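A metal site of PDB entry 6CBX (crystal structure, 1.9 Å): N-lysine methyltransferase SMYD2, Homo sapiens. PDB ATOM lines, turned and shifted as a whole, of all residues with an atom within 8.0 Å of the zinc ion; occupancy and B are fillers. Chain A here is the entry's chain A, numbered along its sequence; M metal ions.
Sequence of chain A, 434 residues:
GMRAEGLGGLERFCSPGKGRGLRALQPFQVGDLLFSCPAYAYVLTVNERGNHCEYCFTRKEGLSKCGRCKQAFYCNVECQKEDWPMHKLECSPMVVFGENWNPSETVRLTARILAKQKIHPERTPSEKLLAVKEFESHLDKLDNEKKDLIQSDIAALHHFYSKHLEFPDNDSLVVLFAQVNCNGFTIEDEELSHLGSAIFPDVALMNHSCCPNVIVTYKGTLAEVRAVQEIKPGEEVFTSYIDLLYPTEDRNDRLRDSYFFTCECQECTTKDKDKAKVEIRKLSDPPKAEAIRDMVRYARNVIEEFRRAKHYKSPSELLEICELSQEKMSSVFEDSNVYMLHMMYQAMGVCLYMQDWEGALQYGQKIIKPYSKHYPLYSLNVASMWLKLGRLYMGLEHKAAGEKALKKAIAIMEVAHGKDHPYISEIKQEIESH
SG of Cys 69 is bound to the zinc ion.
NE2 of His 87 is bound to the zinc ion, 2.2 Å away.
The zinc ion is bound by the side-chain sulfur (SG) of Cys 66, at 2.4 Å.
The zinc ion is bound by SG of Cys 91 (2.4 Å).
The nearest printed residue that does not touch the zinc ion is Arg 68 (4.2 Å).
The side-chain sulfur of Cys 69 lies close to the backbone NH of Gln 71 (3.6 Å).
SG of Cys 66 lies close to N of Arg 68 (3.5 Å).
The backbone carbonyl oxygen (O) of Ala 72 sits at hydrogen-bond distance from the backbone NH (N) of Cys 66.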
ATOM      1  N   LYS A  65      11.443  17.125 -10.282  1.00  0.00           N
ATOM      2  CA  LYS A  65      12.123  17.775 -11.405  1.00  0.00           C
ATOM      3  C   LYS A  65      11.275  18.879 -12.082  1.00  0.00           C
ATOM      4  O   LYS A  65      10.058  18.752 -12.166  1.00  0.00           O
ATOM      5  CB  LYS A  65      12.436  16.683 -12.414  1.00  0.00           C
ATOM      6  CG  LYS A  65      13.395  17.044 -13.496  1.00  0.00           C
ATOM      7  CD  LYS A  65      13.770  15.811 -14.312  1.00  0.00           C
ATOM      8  CE  LYS A  65      14.886  15.023 -13.658  1.00  0.00           C
ATOM      9  NZ  LYS A  65      14.997  13.657 -14.237  1.00  0.00           N
ATOM     10  N   CYS A  66      11.904  19.965 -12.552  1.00  0.00           N
ATOM     11  CA  CYS A  66      11.198  20.978 -13.382  1.00  0.00           C
ATOM     12  C   CYS A  66      10.822  20.330 -14.701  1.00  0.00           C
ATOM     13  O   CYS A  66      11.690  19.839 -15.389  1.00  0.00           O
ATOM     14  CB  CYS A  66      12.085  22.205 -13.702  1.00  0.00           C
ATOM     15  SG  CYS A  66      11.348  23.439 -14.820  1.00  0.00           S
ATOM     16  N   GLY A  67       9.538  20.323 -15.043  1.00  0.00           N
ATOM     17  CA  GLY A  67       9.038  19.655 -16.255  1.00  0.00           C
ATOM     18  C   GLY A  67       9.411  20.394 -17.529  1.00  0.00           C
ATOM     19  O   GLY A  67       9.396  19.809 -18.624  1.00  0.00           O
ATOM     20  N   ARG A  68       9.801  21.671 -17.381  1.00  0.00           N
ATOM     21  CA  ARG A  68      10.083  22.545 -18.505  1.00  0.00           C
ATOM     22  C   ARG A  68      11.507  22.359 -18.987  1.00  0.00           C
ATOM     23  O   ARG A  68      11.720  22.184 -20.170  1.00  0.00           O
ATOM     24  CB  ARG A  68       9.818  24.011 -18.134  1.00  0.00           C
ATOM     25  CG  ARG A  68       8.440  24.265 -17.550  1.00  0.00           C
ATOM     26  CD  ARG A  68       8.293  25.685 -17.065  1.00  0.00           C
ATOM     27  NE  ARG A  68       6.891  25.977 -16.787  1.00  0.00           N
ATOM     28  CZ  ARG A  68       6.356  26.295 -15.612  1.00  0.00           C
ATOM     29  NH1 ARG A  68       5.058  26.542 -15.558  1.00  0.00           N
ATOM     30  NH2 ARG A  68       7.094  26.404 -14.499  1.00  0.00           N
ATOM     31  N   CYS A  69      12.492  22.403 -18.084  1.00  0.00           N
ATOM     32  CA  CYS A  69      13.890  22.166 -18.460  1.00  0.00           C
ATOM     33  C   CYS A  69      14.446  20.817 -18.067  1.00  0.00           C
ATOM     34  O   CYS A  69      15.486  20.424 -18.576  1.00  0.00           O
ATOM     35  CB  CYS A  69      14.824  23.246 -17.876  1.00  0.00           C
ATOM     36  SG  CYS A  69      14.675  23.398 -16.082  1.00  0.00           S
ATOM     37  N   LYS A  70      13.820  20.118 -17.123  1.00  0.00           N
ATOM     38  CA  LYS A  70      14.392  18.869 -16.590  1.00  0.00           C
ATOM     39  C   LYS A  70      15.806  19.000 -15.937  1.00  0.00           C
ATOM     40  O   LYS A  70      16.493  18.005 -15.815  1.00  0.00           O
ATOM     41  CB  LYS A  70      14.374  17.766 -17.679  1.00  0.00           C
ATOM     42  CG  LYS A  70      12.994  17.591 -18.304  1.00  0.00           C
ATOM     43  CD  LYS A  70      12.629  16.133 -18.513  1.00  0.00           C
ATOM     44  CE  LYS A  70      11.228  15.995 -19.102  1.00  0.00           C
ATOM     45  NZ  LYS A  70      11.183  16.552 -20.482  1.00  0.00           N
ATOM     46  N   GLN A  71      16.210  20.200 -15.516  1.00  0.00           N
ATOM     47  CA  GLN A  71      17.520  20.419 -14.864  1.00  0.00           C
ATOM     48  C   GLN A  71      17.416  20.869 -13.422  1.00  0.00           C
ATOM     49  O   GLN A  71      18.334  20.643 -12.644  1.00  0.00           O
ATOM     50  CB  GLN A  71      18.349  21.453 -15.610  1.00  0.00           C
ATOM     51  CG  GLN A  71      18.389  21.282 -17.116  1.00  0.00           C
ATOM     52  CD  GLN A  71      19.473  20.348 -17.597  1.00  0.00           C
ATOM     53  OE1 GLN A  71      19.667  19.261 -17.061  1.00  0.00           O
ATOM     54  NE2 GLN A  71      20.201  20.771 -18.623  1.00  0.00           N
ATOM     55  N   ALA A  72      16.337  21.546 -13.067  1.00  0.00           N
ATOM     56  CA  ALA A  72      16.143  22.049 -11.718  1.00  0.00           C
ATOM     57  C   ALA A  72      15.293  21.051 -10.936  1.00  0.00           C
ATOM     58  O   ALA A  72      14.509  20.273 -11.512  1.00  0.00           O
ATOM     59  CB  ALA A  72      15.487  23.424 -11.753  1.00  0.00           C
ATOM     60  N   PHE A  73      15.469  21.067  -9.619  1.00  0.00           N
ATOM     61  CA  PHE A  73      14.767  20.142  -8.716  1.00  0.00           C
ATOM     62  C   PHE A  73      14.171  20.923  -7.561  1.00  0.00           C
ATOM     63  O   PHE A  73      14.805  21.867  -7.048  1.00  0.00           O
ATOM     64  CB  PHE A  73      15.727  19.067  -8.239  1.00  0.00           C
ATOM     65  CG  PHE A  73      16.139  18.088  -9.306  1.00  0.00           C
ATOM     66  CD1 PHE A  73      17.138  18.406 -10.207  1.00  0.00           C
ATOM     67  CD2 PHE A  73      15.530  16.833  -9.401  1.00  0.00           C
ATOM     68  CE1 PHE A  73      17.530  17.505 -11.196  1.00  0.00           C
ATOM     69  CE2 PHE A  73      15.921  15.916 -10.374  1.00  0.00           C
ATOM     70  CZ  PHE A  73      16.921  16.257 -11.283  1.00  0.00           C
ATOM     71  N   TYR A  74      12.951  20.562  -7.175  1.00  0.00           N
ATOM     72  CA  TYR A  74      12.153  21.286  -6.184  1.00  0.00           C
ATOM     73  C   TYR A  74      11.477  20.360  -5.141  1.00  0.00           C
ATOM     74  O   TYR A  74      11.100  19.221  -5.455  1.00  0.00           O
ATOM     75  CB  TYR A  74      11.075  22.096  -6.904  1.00  0.00           C
ATOM     76  CG  TYR A  74      11.636  23.207  -7.791  1.00  0.00           C
ATOM     77  CD1 TYR A  74      12.166  24.363  -7.230  1.00  0.00           C
ATOM     78  CD2 TYR A  74      11.648  23.074  -9.178  1.00  0.00           C
ATOM     79  CE1 TYR A  74      12.672  25.380  -8.037  1.00  0.00           C
ATOM     80  CE2 TYR A  74      12.155  24.085  -9.992  1.00  0.00           C
ATOM     81  CZ  TYR A  74      12.671  25.228  -9.419  1.00  0.00           C
ATOM     82  OH  TYR A  74      13.163  26.205 -10.242  1.00  0.00           O
ATOM     83  N   GLN A  80       8.765  25.355  -6.498  1.00  0.00           N
ATOM     84  CA  GLN A  80       8.803  25.601  -7.952  1.00  0.00           C
ATOM     85  C   GLN A  80       8.216  26.958  -8.365  1.00  0.00           C
ATOM     86  O   GLN A  80       8.858  27.702  -9.116  1.00  0.00           O
ATOM     87  CB  GLN A  80       8.082  24.506  -8.737  1.00  0.00           C
ATOM     88  CG  GLN A  80       8.221  24.659 -10.242  1.00  0.00           C
ATOM     89  CD  GLN A  80       7.405  23.657 -11.060  1.00  0.00           C
ATOM     90  OE1 GLN A  80       6.442  23.056 -10.583  1.00  0.00           O
ATOM     91  NE2 GLN A  80       7.804  23.481 -12.315  1.00  0.00           N
ATOM     92  N   ASP A  83      10.440  29.943  -6.940  1.00  0.00           N
ATOM     93  CA  ASP A  83      11.738  30.086  -7.631  1.00  0.00           C
ATOM     94  C   ASP A  83      11.658  30.643  -9.052  1.00  0.00           C
ATOM     95  O   ASP A  83      12.692  31.069  -9.611  1.00  0.00           O
ATOM     96  CB  ASP A  83      12.458  28.727  -7.684  1.00  0.00           C
ATOM     97  CG  ASP A  83      13.958  28.833  -7.993  1.00  0.00           C
ATOM     98  OD1 ASP A  83      14.649  29.679  -7.397  1.00  0.00           O
ATOM     99  OD2 ASP A  83      14.484  28.013  -8.798  1.00  0.00           O
ATOM    100  N   TRP A  84      10.464  30.639  -9.652  1.00  0.00           N
ATOM    101  CA  TRP A  84      10.310  30.910 -11.098  1.00  0.00           C
ATOM    102  C   TRP A  84      10.900  32.256 -11.543  1.00  0.00           C
ATOM    103  O   TRP A  84      11.638  32.274 -12.520  1.00  0.00           O
ATOM    104  CB  TRP A  84       8.844  30.782 -11.541  1.00  0.00           C
ATOM    105  CG  TRP A  84       8.624  31.043 -13.033  1.00  0.00           C
ATOM    106  CD1 TRP A  84       8.037  32.135 -13.592  1.00  0.00           C
ATOM    107  CD2 TRP A  84       9.047  30.223 -14.117  1.00  0.00           C
ATOM    108  NE1 TRP A  84       8.043  32.043 -14.963  1.00  0.00           N
ATOM    109  CE2 TRP A  84       8.663  30.871 -15.310  1.00  0.00           C
ATOM    110  CE3 TRP A  84       9.728  28.995 -14.198  1.00  0.00           C
ATOM    111  CZ2 TRP A  84       8.921  30.323 -16.575  1.00  0.00           C
ATOM    112  CZ3 TRP A  84       9.996  28.471 -15.444  1.00  0.00           C
ATOM    113  CH2 TRP A  84       9.572  29.121 -16.625  1.00  0.00           C
ATOM    114  N   HIS A  87      14.450  31.318 -11.670  1.00  0.00           N
ATOM    115  CA  HIS A  87      14.624  30.185 -12.538  1.00  0.00           C
ATOM    116  C   HIS A  87      14.302  30.461 -14.027  1.00  0.00           C
ATOM    117  O   HIS A  87      14.945  29.870 -14.892  1.00  0.00           O
ATOM    118  CB  HIS A  87      13.816  28.987 -12.051  1.00  0.00           C
ATOM    119  CG  HIS A  87      14.065  27.754 -12.850  1.00  0.00           C
ATOM    120  ND1 HIS A  87      15.313  27.219 -13.026  1.00  0.00           N
ATOM    121  CD2 HIS A  87      13.222  26.981 -13.570  1.00  0.00           C
ATOM    122  CE1 HIS A  87      15.233  26.155 -13.800  1.00  0.00           C
ATOM    123  NE2 HIS A  87      13.974  25.993 -14.144  1.00  0.00           N
ATOM    124  N   LYS A  88      13.357  31.352 -14.294  1.00  0.00           N
ATOM    125  CA  LYS A  88      12.960  31.697 -15.680  1.00  0.00           C
ATOM    126  C   LYS A  88      14.116  32.269 -16.499  1.00  0.00           C
ATOM    127  O   LYS A  88      14.094  32.235 -17.730  1.00  0.00           O
ATOM    128  CB  LYS A  88      11.801  32.710 -15.684  1.00  0.00           C
ATOM    129  CG  LYS A  88      12.146  34.119 -15.214  1.00  0.00           C
ATOM    130  CD  LYS A  88      10.977  35.097 -15.451  1.00  0.00           C
ATOM    131  CE  LYS A  88      11.393  36.564 -15.377  1.00  0.00           C
ATOM    132  NZ  LYS A  88      11.846  37.012 -14.045  1.00  0.00           N
ATOM    133  N   GLU A  90      16.986  31.010 -16.658  1.00  0.00           N
ATOM    134  CA  GLU A  90      17.811  29.888 -17.102  1.00  0.00           C
ATOM    135  C   GLU A  90      17.084  28.706 -17.688  1.00  0.00           C
ATOM    136  O   GLU A  90      17.707  27.908 -18.376  1.00  0.00           O
ATOM    137  CB  GLU A  90      18.648  29.379 -15.901  1.00  0.00           C
ATOM    138  CG  GLU A  90      19.579  30.469 -15.383  1.00  0.00           C
ATOM    139  CD  GLU A  90      20.425  30.052 -14.203  1.00  0.00           C
ATOM    140  OE1 GLU A  90      19.987  29.174 -13.423  1.00  0.00           O
ATOM    141  OE2 GLU A  90      21.529  30.643 -14.027  1.00  0.00           O
ATOM    142  N   CYS A  91      15.785  28.587 -17.413  1.00  0.00           N
ATOM    143  CA  CYS A  91      15.011  27.377 -17.731  1.00  0.00           C
ATOM    144  C   CYS A  91      15.040  27.130 -19.245  1.00  0.00           C
ATOM    145  O   CYS A  91      15.598  26.138 -19.713  1.00  0.00           O
ATOM    146  CB  CYS A  91      13.584  27.507 -17.179  1.00  0.00           C
ATOM    147  SG  CYS A  91      12.510  26.082 -17.446  1.00  0.00           S
ATOM    148  N   SER A  92      14.458  28.030 -20.037  1.00  0.00           N
ATOM    149  CA  SER A  92      14.533  27.874 -21.488  1.00  0.00           C
ATOM    150  C   SER A  92      15.976  27.915 -21.999  1.00  0.00           C
ATOM    151  O   SER A  92      16.365  27.039 -22.773  1.00  0.00           O
ATOM    152  CB  SER A  92      13.678  28.891 -22.233  1.00  0.00           C
ATOM    153  OG  SER A  92      13.980  28.826 -23.611  1.00  0.00           O
ATOM    154  N   MET A  94      18.678  26.833 -20.768  1.00  0.00           N
ATOM    155  CA  MET A  94      19.312  25.519 -20.609  1.00  0.00           C
ATOM    156  C   MET A  94      18.825  24.545 -21.703  1.00  0.00           C
ATOM    157  O   MET A  94      19.615  23.747 -22.184  1.00  0.00           O
ATOM    158  CB  MET A  94      19.060  24.941 -19.216  1.00  0.00           C
ATOM    159  CG  MET A  94      19.998  25.546 -18.163  1.00  0.00           C
ATOM    160  SD  MET A  94      19.856  24.809 -16.517  1.00  0.00           S
ATOM    161  CE  MET A  94      18.218  25.339 -16.031  1.00  0.00           C
ATOM    162  N   VAL A  95      17.549  24.637 -22.058  1.00  0.00           N
ATOM    163  CA  VAL A  95      16.992  23.821 -23.151  1.00  0.00           C
ATOM    164  C   VAL A  95      17.641  24.259 -24.471  1.00  0.00           C
ATOM    165  O   VAL A  95      18.183  23.432 -25.199  1.00  0.00           O
ATOM    166  CB  VAL A  95      15.440  23.926 -23.203  1.00  0.00           C
ATOM    167  CG1 VAL A  95      14.871  23.217 -24.430  1.00  0.00           C
ATOM    168  CG2 VAL A  95      14.832  23.354 -21.920  1.00  0.00           C
HETATM  169 ZN    ZN M   1      13.184  24.660 -15.663  1.00  0.00          ZN
